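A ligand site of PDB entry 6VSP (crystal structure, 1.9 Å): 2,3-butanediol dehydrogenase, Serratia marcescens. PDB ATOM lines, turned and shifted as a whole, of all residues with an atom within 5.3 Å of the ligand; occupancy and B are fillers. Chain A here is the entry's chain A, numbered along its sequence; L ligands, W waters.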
ATOM      1  N   GLY A  25      32.854 -14.567  -8.126  1.00  0.00           N
ATOM      2  CA  GLY A  25      32.603 -13.219  -7.582  1.00  0.00           C
ATOM      3  C   GLY A  25      32.377 -13.268  -6.087  1.00  0.00           C
ATOM      4  O   GLY A  25      31.577 -12.448  -5.582  1.00  0.00           O
ATOM      5  N   ALA A  26      33.094 -14.147  -5.384  1.00  0.00           N
ATOM      6  CA  ALA A  26      32.882 -14.419  -3.941  1.00  0.00           C
ATOM      7  C   ALA A  26      33.565 -13.364  -3.063  1.00  0.00           C
ATOM      8  O   ALA A  26      33.327 -13.412  -1.846  1.00  0.00           O
ATOM      9  CB  ALA A  26      33.338 -15.798  -3.571  1.00  0.00           C
ATOM     10  N   GLY A  27      34.343 -12.423  -3.631  1.00  0.00           N
ATOM     11  CA  GLY A  27      35.155 -11.467  -2.864  1.00  0.00           C
ATOM     12  C   GLY A  27      34.357 -10.256  -2.400  1.00  0.00           C
ATOM     13  O   GLY A  27      34.863  -9.483  -1.553  1.00  0.00           O
ATOM     14  N   ASN A  28      33.121 -10.093  -2.893  1.00  0.00           N
ATOM     15  CA  ASN A  28      32.295  -8.892  -2.632  1.00  0.00           C
ATOM     16  C   ASN A  28      30.819  -9.194  -2.837  1.00  0.00           C
ATOM     17  O   ASN A  28      30.511 -10.223  -3.454  1.00  0.00           O
ATOM     18  CB  ASN A  28      32.641  -7.753  -3.575  1.00  0.00           C
ATOM     19  CG  ASN A  28      34.041  -7.205  -3.387  1.00  0.00           C
ATOM     20  OD1 ASN A  28      34.937  -7.537  -4.149  1.00  0.00           O
ATOM     21  ND2 ASN A  28      34.191  -6.351  -2.409  1.00  0.00           N
ATOM     22  N   GLY A  29      29.948  -8.329  -2.293  1.00  0.00           N
ATOM     23  CA  GLY A  29      28.521  -8.249  -2.635  1.00  0.00           C
ATOM     24  C   GLY A  29      27.808  -9.577  -2.477  1.00  0.00           C
ATOM     25  O   GLY A  29      27.904 -10.216  -1.412  1.00  0.00           O
ATOM     26  N   MET A  30      27.032  -9.964  -3.483  1.00  0.00           N
ATOM     27  CA  MET A  30      26.129 -11.124  -3.373  1.00  0.00           C
ATOM     28  C   MET A  30      26.941 -12.419  -3.278  1.00  0.00           C
ATOM     29  O   MET A  30      26.547 -13.290  -2.488  1.00  0.00           O
ATOM     30  CB  MET A  30      25.152 -11.138  -4.555  1.00  0.00           C
ATOM     31  CG  MET A  30      24.018 -10.156  -4.345  1.00  0.00           C
ATOM     32  SD  MET A  30      22.881 -10.153  -5.711  1.00  0.00           S
ATOM     33  CE  MET A  30      23.620  -8.897  -6.760  1.00  0.00           C
ATOM     34  N   GLY A  31      28.064 -12.513  -4.001  1.00  0.00           N
ATOM     35  CA  GLY A  31      28.996 -13.655  -3.902  1.00  0.00           C
ATOM     36  C   GLY A  31      29.501 -13.847  -2.471  1.00  0.00           C
ATOM     37  O   GLY A  31      29.490 -15.002  -1.966  1.00  0.00           O
ATOM     38  N   ALA A  48      36.056 -17.974  -5.735  1.00  0.00           N
ATOM     39  CA  ALA A  48      36.747 -17.626  -6.991  1.00  0.00           C
ATOM     40  C   ALA A  48      36.525 -16.136  -7.261  1.00  0.00           C
ATOM     41  O   ALA A  48      35.338 -15.686  -7.259  1.00  0.00           O
ATOM     42  CB  ALA A  48      36.255 -18.471  -8.125  1.00  0.00           C
ATOM     43  N   ASP A  49      37.615 -15.393  -7.447  1.00  0.00           N
ATOM     44  CA  ASP A  49      37.523 -13.953  -7.756  1.00  0.00           C
ATOM     45  C   ASP A  49      38.850 -13.495  -8.321  1.00  0.00           C
ATOM     46  O   ASP A  49      39.919 -14.137  -8.029  1.00  0.00           O
ATOM     47  CB  ASP A  49      37.119 -13.151  -6.524  1.00  0.00           C
ATOM     48  CG  ASP A  49      36.369 -11.873  -6.840  1.00  0.00           C
ATOM     49  OD1 ASP A  49      36.917 -10.983  -7.530  1.00  0.00           O
ATOM     50  OD2 ASP A  49      35.212 -11.774  -6.357  1.00  0.00           O
ATOM     51  N   TRP A  50      38.792 -12.438  -9.131  1.00  0.00           N
ATOM     52  CA  TRP A  50      40.010 -11.807  -9.691  1.00  0.00           C
ATOM     53  C   TRP A  50      40.483 -10.667  -8.790  1.00  0.00           C
ATOM     54  O   TRP A  50      41.583 -10.154  -9.051  1.00  0.00           O
ATOM     55  CB  TRP A  50      39.802 -11.411 -11.171  1.00  0.00           C
ATOM     56  CG  TRP A  50      38.816 -10.321 -11.495  1.00  0.00           C
ATOM     57  CD1 TRP A  50      37.983  -9.628 -10.665  1.00  0.00           C
ATOM     58  CD2 TRP A  50      38.581  -9.815 -12.812  1.00  0.00           C
ATOM     59  NE1 TRP A  50      37.242  -8.735 -11.381  1.00  0.00           N
ATOM     60  CE2 TRP A  50      37.588  -8.823 -12.708  1.00  0.00           C
ATOM     61  CE3 TRP A  50      39.120 -10.107 -14.073  1.00  0.00           C
ATOM     62  CZ2 TRP A  50      37.134  -8.099 -13.824  1.00  0.00           C
ATOM     63  CZ3 TRP A  50      38.661  -9.410 -15.176  1.00  0.00           C
ATOM     64  CH2 TRP A  50      37.693  -8.421 -15.045  1.00  0.00           C
ATOM     65  N   ALA A  51      39.698 -10.295  -7.762  1.00  0.00           N
ATOM     66  CA  ALA A  51      40.078  -9.320  -6.713  1.00  0.00           C
ATOM     67  C   ALA A  51      40.729 -10.091  -5.572  1.00  0.00           C
ATOM     68  O   ALA A  51      39.995 -10.594  -4.721  1.00  0.00           O
ATOM     69  CB  ALA A  51      38.875  -8.540  -6.211  1.00  0.00           C
ATOM     70  N   ILE A  72      41.232 -15.965  -9.934  1.00  0.00           N
ATOM     71  CA  ILE A  72      40.907 -16.390 -11.319  1.00  0.00           C
ATOM     72  C   ILE A  72      40.016 -15.335 -11.973  1.00  0.00           C
ATOM     73  O   ILE A  72      39.149 -14.747 -11.283  1.00  0.00           O
ATOM     74  CB  ILE A  72      40.236 -17.765 -11.336  1.00  0.00           C
ATOM     75  CG1 ILE A  72      39.975 -18.242 -12.760  1.00  0.00           C
ATOM     76  CG2 ILE A  72      38.955 -17.769 -10.515  1.00  0.00           C
ATOM     77  CD1 ILE A  72      39.465 -19.641 -12.833  1.00  0.00           C
ATOM     78  N   ASP A  73      40.266 -15.133 -13.265  1.00  0.00           N
ATOM     79  CA  ASP A  73      39.406 -14.411 -14.239  1.00  0.00           C
ATOM     80  C   ASP A  73      38.519 -15.449 -14.927  1.00  0.00           C
ATOM     81  O   ASP A  73      39.051 -16.195 -15.750  1.00  0.00           O
ATOM     82  CB  ASP A  73      40.291 -13.671 -15.244  1.00  0.00           C
ATOM     83  CG  ASP A  73      39.507 -12.887 -16.283  1.00  0.00           C
ATOM     84  OD1 ASP A  73      38.269 -13.055 -16.370  1.00  0.00           O
ATOM     85  OD2 ASP A  73      40.129 -12.055 -16.953  1.00  0.00           O
ATOM     86  N   VAL A  74      37.229 -15.497 -14.574  1.00  0.00           N
ATOM     87  CA  VAL A  74      36.272 -16.514 -15.092  1.00  0.00           C
ATOM     88  C   VAL A  74      36.102 -16.386 -16.611  1.00  0.00           C
ATOM     89  O   VAL A  74      35.573 -17.366 -17.185  1.00  0.00           O
ATOM     90  CB  VAL A  74      34.896 -16.459 -14.417  1.00  0.00           C
ATOM     91  CG1 VAL A  74      35.008 -16.849 -12.951  1.00  0.00           C
ATOM     92  CG2 VAL A  74      34.199 -15.112 -14.598  1.00  0.00           C
ATOM     93  N   SER A  75      36.506 -15.280 -17.242  1.00  0.00           N
ATOM     94  CA  SER A  75      36.441 -15.124 -18.736  1.00  0.00           C
ATOM     95  C   SER A  75      37.457 -16.035 -19.439  1.00  0.00           C
ATOM     96  O   SER A  75      37.346 -16.199 -20.655  1.00  0.00           O
ATOM     97  CB  SER A  75      36.626 -13.703 -19.184  1.00  0.00           C
ATOM     98  OG  SER A  75      37.981 -13.297 -19.115  1.00  0.00           O
ATOM     99  N   ASN A 100      28.241 -16.216 -10.307  1.00  0.00           N
ATOM    100  CA  ASN A 100      27.846 -14.902  -9.762  1.00  0.00           C
ATOM    101  C   ASN A 100      28.729 -13.767 -10.287  1.00  0.00           C
ATOM    102  O   ASN A 100      28.229 -12.625 -10.338  1.00  0.00           O
ATOM    103  CB  ASN A 100      27.730 -15.007  -8.241  1.00  0.00           C
ATOM    104  CG  ASN A 100      27.550 -13.668  -7.582  1.00  0.00           C
ATOM    105  OD1 ASN A 100      26.414 -13.195  -7.526  1.00  0.00           O
ATOM    106  ND2 ASN A 100      28.659 -13.054  -7.172  1.00  0.00           N
ATOM    107  N   ALA A 101      29.998 -14.035 -10.634  1.00  0.00           N
ATOM    108  CA  ALA A 101      30.946 -13.001 -11.100  1.00  0.00           C
ATOM    109  C   ALA A 101      30.304 -12.266 -12.267  1.00  0.00           C
ATOM    110  O   ALA A 101      29.720 -12.924 -13.167  1.00  0.00           O
ATOM    111  CB  ALA A 101      32.263 -13.583 -11.548  1.00  0.00           C
ATOM    112  N   GLY A 102      30.431 -10.956 -12.239  1.00  0.00           N
ATOM    113  CA  GLY A 102      29.823 -10.075 -13.229  1.00  0.00           C
ATOM    114  C   GLY A 102      30.385  -8.695 -13.139  1.00  0.00           C
ATOM    115  O   GLY A 102      30.857  -8.298 -12.026  1.00  0.00           O
ATOM    116  N   VAL A 103      30.357  -7.997 -14.280  1.00  0.00           N
ATOM    117  CA  VAL A 103      30.672  -6.557 -14.386  1.00  0.00           C
ATOM    118  C   VAL A 103      29.526  -5.842 -15.101  1.00  0.00           C
ATOM    119  O   VAL A 103      28.757  -6.496 -15.862  1.00  0.00           O
ATOM    120  CB  VAL A 103      32.006  -6.295 -15.099  1.00  0.00           C
ATOM    121  CG1 VAL A 103      33.192  -6.824 -14.301  1.00  0.00           C
ATOM    122  CG2 VAL A 103      32.017  -6.858 -16.513  1.00  0.00           C
ATOM    123  N   VAL A 123      33.101 -11.723 -19.244  1.00  0.00           N
ATOM    124  CA  VAL A 123      32.783 -12.053 -17.827  1.00  0.00           C
ATOM    125  C   VAL A 123      31.358 -12.591 -17.738  1.00  0.00           C
ATOM    126  O   VAL A 123      31.184 -13.656 -17.194  1.00  0.00           O
ATOM    127  CB  VAL A 123      33.006 -10.860 -16.888  1.00  0.00           C
ATOM    128  CG1 VAL A 123      32.697 -11.221 -15.451  1.00  0.00           C
ATOM    129  CG2 VAL A 123      34.422 -10.335 -17.023  1.00  0.00           C
ATOM    130  N   ASP A 124      30.377 -11.827 -18.247  1.00  0.00           N
ATOM    131  CA  ASP A 124      28.942 -12.009 -17.930  1.00  0.00           C
ATOM    132  C   ASP A 124      28.354 -13.154 -18.748  1.00  0.00           C
ATOM    133  O   ASP A 124      27.368 -13.729 -18.271  1.00  0.00           O
ATOM    134  CB  ASP A 124      28.152 -10.694 -18.106  1.00  0.00           C
ATOM    135  CG  ASP A 124      28.592  -9.549 -17.189  1.00  0.00           C
ATOM    136  OD1 ASP A 124      29.467  -9.785 -16.361  1.00  0.00           O
ATOM    137  OD2 ASP A 124      28.022  -8.436 -17.313  1.00  0.00           O
ATOM    138  N   THR A 149      23.712 -16.151 -11.335  1.00  0.00           N
ATOM    139  CA  THR A 149      23.240 -14.780 -11.037  1.00  0.00           C
ATOM    140  C   THR A 149      22.971 -14.094 -12.369  1.00  0.00           C
ATOM    141  O   THR A 149      23.909 -13.566 -12.953  1.00  0.00           O
ATOM    142  CB  THR A 149      24.187 -13.934 -10.181  1.00  0.00           C
ATOM    143  OG1 THR A 149      24.545 -14.706  -9.035  1.00  0.00           O
ATOM    144  CG2 THR A 149      23.516 -12.626  -9.788  1.00  0.00           C
ATOM    145  N   ALA A 150      21.729 -14.058 -12.800  1.00  0.00           N
ATOM    146  CA  ALA A 150      21.342 -13.275 -13.991  1.00  0.00           C
ATOM    147  C   ALA A 150      21.018 -11.862 -13.508  1.00  0.00           C
ATOM    148  O   ALA A 150      21.872 -11.277 -12.829  1.00  0.00           O
ATOM    149  CB  ALA A 150      20.193 -13.957 -14.711  1.00  0.00           C
ATOM    150  N   SER A 151      19.828 -11.354 -13.818  1.00  0.00           N
ATOM    151  CA  SER A 151      19.386  -9.978 -13.480  1.00  0.00           C
ATOM    152  C   SER A 151      17.975  -9.835 -14.028  1.00  0.00           C
ATOM    153  O   SER A 151      17.694 -10.505 -15.003  1.00  0.00           O
ATOM    154  CB  SER A 151      20.298  -8.910 -14.078  1.00  0.00           C
ATOM    155  OG  SER A 151      19.788  -7.609 -13.745  1.00  0.00           O
ATOM    156  N   VAL A 152      17.160  -8.924 -13.498  1.00  0.00           N
ATOM    157  CA  VAL A 152      15.959  -8.448 -14.249  1.00  0.00           C
ATOM    158  C   VAL A 152      16.414  -7.957 -15.640  1.00  0.00           C
ATOM    159  O   VAL A 152      15.618  -8.067 -16.596  1.00  0.00           O
ATOM    160  CB  VAL A 152      15.156  -7.382 -13.459  1.00  0.00           C
ATOM    161  CG1 VAL A 152      14.651  -7.994 -12.179  1.00  0.00           C
ATOM    162  CG2 VAL A 152      15.974  -6.101 -13.166  1.00  0.00           C
ATOM    163  N   TYR A 164      25.197  -5.136 -21.389  1.00  0.00           N
ATOM    164  CA  TYR A 164      24.836  -5.835 -20.131  1.00  0.00           C
ATOM    165  C   TYR A 164      23.531  -6.615 -20.323  1.00  0.00           C
ATOM    166  O   TYR A 164      23.442  -7.767 -19.933  1.00  0.00           O
ATOM    167  CB  TYR A 164      24.703  -4.838 -18.981  1.00  0.00           C
ATOM    168  CG  TYR A 164      24.417  -5.439 -17.635  1.00  0.00           C
ATOM    169  CD1 TYR A 164      25.427  -6.071 -16.932  1.00  0.00           C
ATOM    170  CD2 TYR A 164      23.189  -5.279 -17.033  1.00  0.00           C
ATOM    171  CE1 TYR A 164      25.195  -6.583 -15.659  1.00  0.00           C
ATOM    172  CE2 TYR A 164      22.941  -5.788 -15.767  1.00  0.00           C
ATOM    173  CZ  TYR A 164      23.955  -6.436 -15.081  1.00  0.00           C
ATOM    174  OH  TYR A 164      23.745  -6.895 -13.815  1.00  0.00           O
ATOM    175  N   LYS A 168      23.051 -10.612 -20.005  1.00  0.00           N
ATOM    176  CA  LYS A 168      22.153 -11.212 -19.012  1.00  0.00           C
ATOM    177  C   LYS A 168      21.036 -11.961 -19.740  1.00  0.00           C
ATOM    178  O   LYS A 168      20.552 -12.966 -19.167  1.00  0.00           O
ATOM    179  CB  LYS A 168      21.685 -10.137 -18.026  1.00  0.00           C
ATOM    180  CG  LYS A 168      22.767  -9.601 -17.090  1.00  0.00           C
ATOM    181  CD  LYS A 168      23.390 -10.688 -16.243  1.00  0.00           C
ATOM    182  CE  LYS A 168      24.238 -10.127 -15.130  1.00  0.00           C
ATOM    183  NZ  LYS A 168      24.994 -11.163 -14.394  1.00  0.00           N
ATOM    184  N   PRO A 194      18.004 -10.538  -9.733  1.00  0.00           N
ATOM    185  CA  PRO A 194      17.776  -9.381  -8.864  1.00  0.00           C
ATOM    186  C   PRO A 194      17.543  -8.120  -9.679  1.00  0.00           C
ATOM    187  O   PRO A 194      18.016  -8.018 -10.828  1.00  0.00           O
ATOM    188  CB  PRO A 194      19.086  -9.240  -8.056  1.00  0.00           C
ATOM    189  CG  PRO A 194      19.818 -10.550  -8.309  1.00  0.00           C
ATOM    190  CD  PRO A 194      19.399 -10.990  -9.694  1.00  0.00           C
ATOM    191  N   SER A 195      16.824  -7.162  -9.093  1.00  0.00           N
ATOM    192  CA  SER A 195      16.834  -5.744  -9.514  1.00  0.00           C
ATOM    193  C   SER A 195      17.929  -5.048  -8.694  1.00  0.00           C
ATOM    194  O   SER A 195      18.967  -5.705  -8.457  1.00  0.00           O
ATOM    195  CB  SER A 195      15.481  -5.057  -9.419  1.00  0.00           C
ATOM    196  OG  SER A 195      15.563  -3.733  -9.950  1.00  0.00           O
ATOM    197  N   LEU A 196      17.728  -3.797  -8.268  1.00  0.00           N
ATOM    198  CA  LEU A 196      18.787  -3.057  -7.545  1.00  0.00           C
ATOM    199  C   LEU A 196      19.170  -3.776  -6.254  1.00  0.00           C
ATOM    200  O   LEU A 196      18.289  -4.085  -5.449  1.00  0.00           O
ATOM    201  CB  LEU A 196      18.288  -1.639  -7.247  1.00  0.00           C
ATOM    202  CG  LEU A 196      19.308  -0.734  -6.597  1.00  0.00           C
ATOM    203  CD1 LEU A 196      20.547  -0.643  -7.465  1.00  0.00           C
ATOM    204  CD2 LEU A 196      18.703   0.650  -6.370  1.00  0.00           C
ATOM    205  N   VAL A 197      20.450  -4.072  -6.075  1.00  0.00           N
ATOM    206  CA  VAL A 197      21.038  -4.653  -4.821  1.00  0.00           C
ATOM    207  C   VAL A 197      22.139  -3.702  -4.340  1.00  0.00           C
ATOM    208  O   VAL A 197      22.886  -3.183  -5.198  1.00  0.00           O
ATOM    209  CB  VAL A 197      21.585  -6.068  -5.094  1.00  0.00           C
ATOM    210  CG1 VAL A 197      22.002  -6.761  -3.821  1.00  0.00           C
ATOM    211  CG2 VAL A 197      20.534  -6.905  -5.843  1.00  0.00           C
ATOM    212  N   LYS A 198      22.281  -3.546  -3.024  1.00  0.00           N
ATOM    213  CA  LYS A 198      23.307  -2.654  -2.423  1.00  0.00           C
ATOM    214  C   LYS A 198      24.692  -3.295  -2.463  1.00  0.00           C
ATOM    215  O   LYS A 198      25.063  -3.917  -1.469  1.00  0.00           O
ATOM    216  CB  LYS A 198      22.928  -2.379  -0.980  1.00  0.00           C
ATOM    217  CG  LYS A 198      21.676  -1.544  -0.815  1.00  0.00           C
ATOM    218  CD  LYS A 198      21.377  -1.382   0.650  1.00  0.00           C
ATOM    219  CE  LYS A 198      19.974  -0.904   0.945  1.00  0.00           C
ATOM    220  NZ  LYS A 198      19.781  -0.754   2.399  1.00  0.00           N
ATOM    221  N   THR A 199      25.413  -3.102  -3.565  1.00  0.00           N
ATOM    222  CA  THR A 199      26.752  -3.671  -3.797  1.00  0.00           C
ATOM    223  C   THR A 199      27.618  -2.625  -4.492  1.00  0.00           C
ATOM    224  O   THR A 199      27.073  -1.588  -4.961  1.00  0.00           O
ATOM    225  CB  THR A 199      26.700  -4.951  -4.655  1.00  0.00           C
ATOM    226  OG1 THR A 199      26.457  -4.585  -6.000  1.00  0.00           O
ATOM    227  CG2 THR A 199      25.657  -5.949  -4.204  1.00  0.00           C
ATOM    228  N   ASN A 200      28.920  -2.958  -4.599  1.00  0.00           N
ATOM    229  CA  ASN A 200      29.926  -2.225  -5.399  1.00  0.00           C
ATOM    230  C   ASN A 200      29.442  -1.993  -6.841  1.00  0.00           C
ATOM    231  O   ASN A 200      29.797  -0.963  -7.415  1.00  0.00           O
ATOM    232  CB  ASN A 200      31.292  -2.916  -5.378  1.00  0.00           C
ATOM    233  CG  ASN A 200      31.990  -2.776  -4.040  1.00  0.00           C
ATOM    234  OD1 ASN A 200      31.607  -1.943  -3.199  1.00  0.00           O
ATOM    235  ND2 ASN A 200      33.062  -3.528  -3.843  1.00  0.00           N
ATOM    236  N   MET A 201      28.662  -2.897  -7.422  1.00  0.00           N
ATOM    237  CA  MET A 201      28.190  -2.733  -8.825  1.00  0.00           C
ATOM    238  C   MET A 201      27.375  -1.440  -8.974  1.00  0.00           C
ATOM    239  O   MET A 201      27.513  -0.783 -10.016  1.00  0.00           O
ATOM    240  CB  MET A 201      27.383  -3.943  -9.319  1.00  0.00           C
ATOM    241  CG  MET A 201      27.063  -3.868 -10.780  1.00  0.00           C
ATOM    242  SD  MET A 201      26.621  -5.440 -11.531  1.00  0.00           S
ATOM    243  CE  MET A 201      28.231  -6.209 -11.708  1.00  0.00           C
ATOM    244  N   THR A 202      26.580  -1.038  -7.965  1.00  0.00           N
ATOM    245  CA  THR A 202      25.633   0.107  -8.071  1.00  0.00           C
ATOM    246  C   THR A 202      25.929   1.258  -7.117  1.00  0.00           C
ATOM    247  O   THR A 202      25.152   2.206  -7.128  1.00  0.00           O
ATOM    248  CB  THR A 202      24.231  -0.442  -7.807  1.00  0.00           C
ATOM    249  OG1 THR A 202      24.307  -1.034  -6.528  1.00  0.00           O
ATOM    250  CG2 THR A 202      23.830  -1.470  -8.850  1.00  0.00           C
HETATM  251  P1  LIG L   1      30.161  -6.775  -6.627  1.00  0.00           P
HETATM  252  O1  LIG L   1      31.006  -5.798  -7.398  1.00  0.00           O
HETATM  253  O2  LIG L   1      29.855  -6.595  -5.208  1.00  0.00           O
HETATM  254  O3  LIG L   1      30.724  -8.274  -6.793  1.00  0.00           O
HETATM  255  C1  LIG L   1      31.071  -8.775  -8.056  1.00  0.00           C
HETATM  256  C2  LIG L   1      32.304  -9.594  -7.834  1.00  0.00           C
HETATM  257  O4  LIG L   1      32.659 -10.278  -9.068  1.00  0.00           O
HETATM  258  C3  LIG L   1      33.534  -8.766  -7.419  1.00  0.00           C
HETATM  259  O5  LIG L   1      34.196  -9.334  -6.280  1.00  0.00           O
HETATM  260  C4  LIG L   1      34.433  -8.816  -8.660  1.00  0.00           C
HETATM  261  O6  LIG L   1      35.790  -8.611  -8.343  1.00  0.00           O
HETATM  262  C5  LIG L   1      34.057 -10.193  -9.210  1.00  0.00           C
HETATM  263  N1  LIG L   1      34.388 -10.373 -10.612  1.00  0.00           N
HETATM  264  C6  LIG L   1      34.085  -9.543 -11.659  1.00  0.00           C
HETATM  265  N2  LIG L   1      34.518  -9.963 -12.809  1.00  0.00           N
HETATM  266  C7  LIG L   1      35.203 -11.133 -12.509  1.00  0.00           C
HETATM  267  C8  LIG L   1      35.938 -12.028 -13.300  1.00  0.00           C
HETATM  268  N3  LIG L   1      36.149 -11.855 -14.607  1.00  0.00           N
HETATM  269  N4  LIG L   1      36.494 -13.089 -12.680  1.00  0.00           N
HETATM  270  C9  LIG L   1      36.329 -13.226 -11.356  1.00  0.00           C
HETATM  271  N5  LIG L   1      35.680 -12.440 -10.511  1.00  0.00           N
HETATM  272  C10 LIG L   1      35.128 -11.395 -11.149  1.00  0.00           C
HETATM  273  O7  LIG L   1      28.755  -6.767  -7.387  1.00  0.00           O
HETATM  274  P2  LIG L   1      27.471  -7.705  -7.263  1.00  0.00           P
HETATM  275  O8  LIG L   1      27.481  -8.543  -5.998  1.00  0.00           O
HETATM  276  O9  LIG L   1      26.303  -6.798  -7.452  1.00  0.00           O
HETATM  277  O10 LIG L   1      27.644  -8.612  -8.571  1.00  0.00           O
HETATM  278  C11 LIG L   1      27.336  -9.999  -8.554  1.00  0.00           C
HETATM  279  C12 LIG L   1      26.396 -10.375  -9.680  1.00  0.00           C
HETATM  280  O11 LIG L   1      25.089  -9.799  -9.430  1.00  0.00           O
HETATM  281  C13 LIG L   1      26.808  -9.966 -11.106  1.00  0.00           C
HETATM  282  O12 LIG L   1      26.661 -11.007 -12.087  1.00  0.00           O
HETATM  283  C14 LIG L   1      25.833  -8.837 -11.374  1.00  0.00           C
HETATM  284  O13 LIG L   1      25.693  -8.626 -12.772  1.00  0.00           O
HETATM  285  C15 LIG L   1      24.594  -9.377 -10.660  1.00  0.00           C
HETATM  286  N6  LIG L   1      23.546  -8.361 -10.419  1.00  0.00           N
HETATM  287  C16 LIG L   1      23.822  -7.205  -9.708  1.00  0.00           C
HETATM  288  C17 LIG L   1      22.781  -6.339  -9.362  1.00  0.00           C
HETATM  289  C18 LIG L   1      22.970  -5.149  -8.451  1.00  0.00           C
HETATM  290  O14 LIG L   1      22.104  -4.276  -8.422  1.00  0.00           O
HETATM  291  N7  LIG L   1      24.045  -5.149  -7.656  1.00  0.00           N
HETATM  292  C19 LIG L   1      21.501  -6.582  -9.889  1.00  0.00           C
HETATM  293  C20 LIG L   1      21.291  -7.675 -10.686  1.00  0.00           C
HETATM  294  C21 LIG L   1      22.293  -8.584 -10.879  1.00  0.00           C
HETATM  295  O   HOH W   1      33.478  -5.220  -6.479  1.00  0.00           O
HETATM  296  O   HOH W   2      27.293 -13.949 -13.341  1.00  0.00           O
HETATM  297  O   HOH W   3      35.936  -6.243  -7.543  1.00  0.00           O
HETATM  298  O   HOH W   4      29.139 -10.681  -5.972  1.00  0.00           O
HETATM  299  O   HOH W   5      35.419  -6.334 -10.940  1.00  0.00           O
HETATM  300  O   HOH W   6      29.776  -5.189  -2.991  1.00  0.00           O
HETATM  301  O   HOH W   7      32.586  -6.524 -10.743  1.00  0.00           O
HETATM  302  O   HOH W   8      31.137  -4.461  -9.537  1.00  0.00           O
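The backbone carbonyl oxygen (O) of Ile 72 sits close to a nitrogen (N4) of the ligand, 3.4 Å away.
O of Ser 195 sits close to O14 of the ligand (3.4 Å).
Merely in contact with the ligand: Gly 25, Gly 27, Ala 51, Ala 101, Gly 102, Val 103, Val 123, Thr 149, Ala 150, Ser 151, Pro 194, Leu 196, Asn 200 and Thr 202.
Hydrophobic or aromatic side chains that line the ligand: Met 30, Trp 50, Ala 51, Val 74, Ala 101, Val 103, Val 123, Tyr 164, Pro 194, Val 197 and Met 201.
Within 4 Å of the ligand: Gly 25, Gly 27, Asn 28, Gly 29, Met 30, Asp 49, Trp 50, Ala 51, Ile 72, Asp 73, Val 74, Asn 100, Ala 101, Gly 102, Val 103, Val 123, Thr 149, Ala 150, Ser 151, Tyr 164, Lys 168, Pro 194, Ser 195, Leu 196, Val 197, Thr 199, Asn 200, Met 201 and Thr 202.
The nearest printed residue that does not touch the ligand is Ser 75 (4.3 Å).
Water W6 lies within hydrogen-bond range of an oxygen (O2) of the ligand, the backbone NH (N) of Asn 200 and the backbone NH (N) of Gly 29.
Water W1 bridges an oxygen (O1) of the ligand (2.7 Å) and the side-chain amide nitrogen (ND2) of Asn 200 (3.2 Å).
Water W5 bridges the indole nitrogen (NE1) of Trp 50 (3.0 Å) and an oxygen (O6) of the ligand (3.5 Å).
O9 of the ligand is in hydrogen-bond range of OG1 of Thr 199 (2.7 Å).
An oxygen (O2) of the ligand lies close to the backbone NH (N) of Gly 29 (3.4 Å).
The backbone carbonyl oxygen (O) of Asn 100 lies within hydrogen-bond range of an oxygen (O12) of the ligand, 2.9 Å away.
The backbone NH (N) of Trp 50 is in hydrogen-bond range of a nitrogen (N5) of the ligand.
A nitrogen (N4) of the ligand sits at hydrogen-bond distance from the backbone NH (N) of Val 74, 3.2 Å away.
NE1 of Trp 50 lies close to N2 of the ligand, at 3.3 Å.
OD2 of Asp 49 sits at hydrogen-bond distance from O5 of the ligand, at 2.6 Å.
The side-chain amide oxygen (OD1) of Asn 28 lies within hydrogen-bond range of an oxygen (O5) of the ligand.
OD1 of Asp 73 sits at hydrogen-bond distance from N3 of the ligand, at 3.0 Å.
An oxygen (O13) of the ligand lies close to the side-chain sulfur of Met 201.
OH of Tyr 164 is in hydrogen-bond range of O13 of the ligand, 2.8 Å away.
The side-chain amino group (NZ) of Lys 168 lies within hydrogen-bond range of an oxygen (O12) of the ligand (2.9 Å).
O14 of the ligand lies within hydrogen-bond range of N of Val 197, at 2.9 Å.
An oxygen (O8) of the ligand lies within hydrogen-bond range of the backbone NH (N) of Met 30 (2.9 Å).
N7 of the ligand lies within hydrogen-bond range of O of Val 197 (3.4 Å).
The side-chain amino group (NZ) of Lys 168 sits at hydrogen-bond distance from the backbone carbonyl oxygen (O) of Thr 149 (3.0 Å).
ND2 of Asn 100 is in hydrogen-bond range of O of Gly 25 (3.4 Å).
The side-chain carboxylate (OD2) of Asp 49 lies within hydrogen-bond range of the backbone NH (N) of Ala 26.
The side-chain carboxylate of Asp 73 sits at hydrogen-bond distance from the side-chain hydroxyl of Ser 75 (2.8 Å).
The backbone carbonyl oxygen (O) of Val 197 is in hydrogen-bond range of the side-chain hydroxyl (OG1) of Thr 202 (2.9 Å).
N of Gly 27 sits at hydrogen-bond distance from OD2 of Asp 49 (2.9 Å).
ND2 of Asn 100 sits close to N of Gly 31 (3.3 Å).
The backbone carbonyl oxygen (O) of Ala 48 sits at hydrogen-bond distance from the backbone NH (N) of Gly 25, at 2.9 Å.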
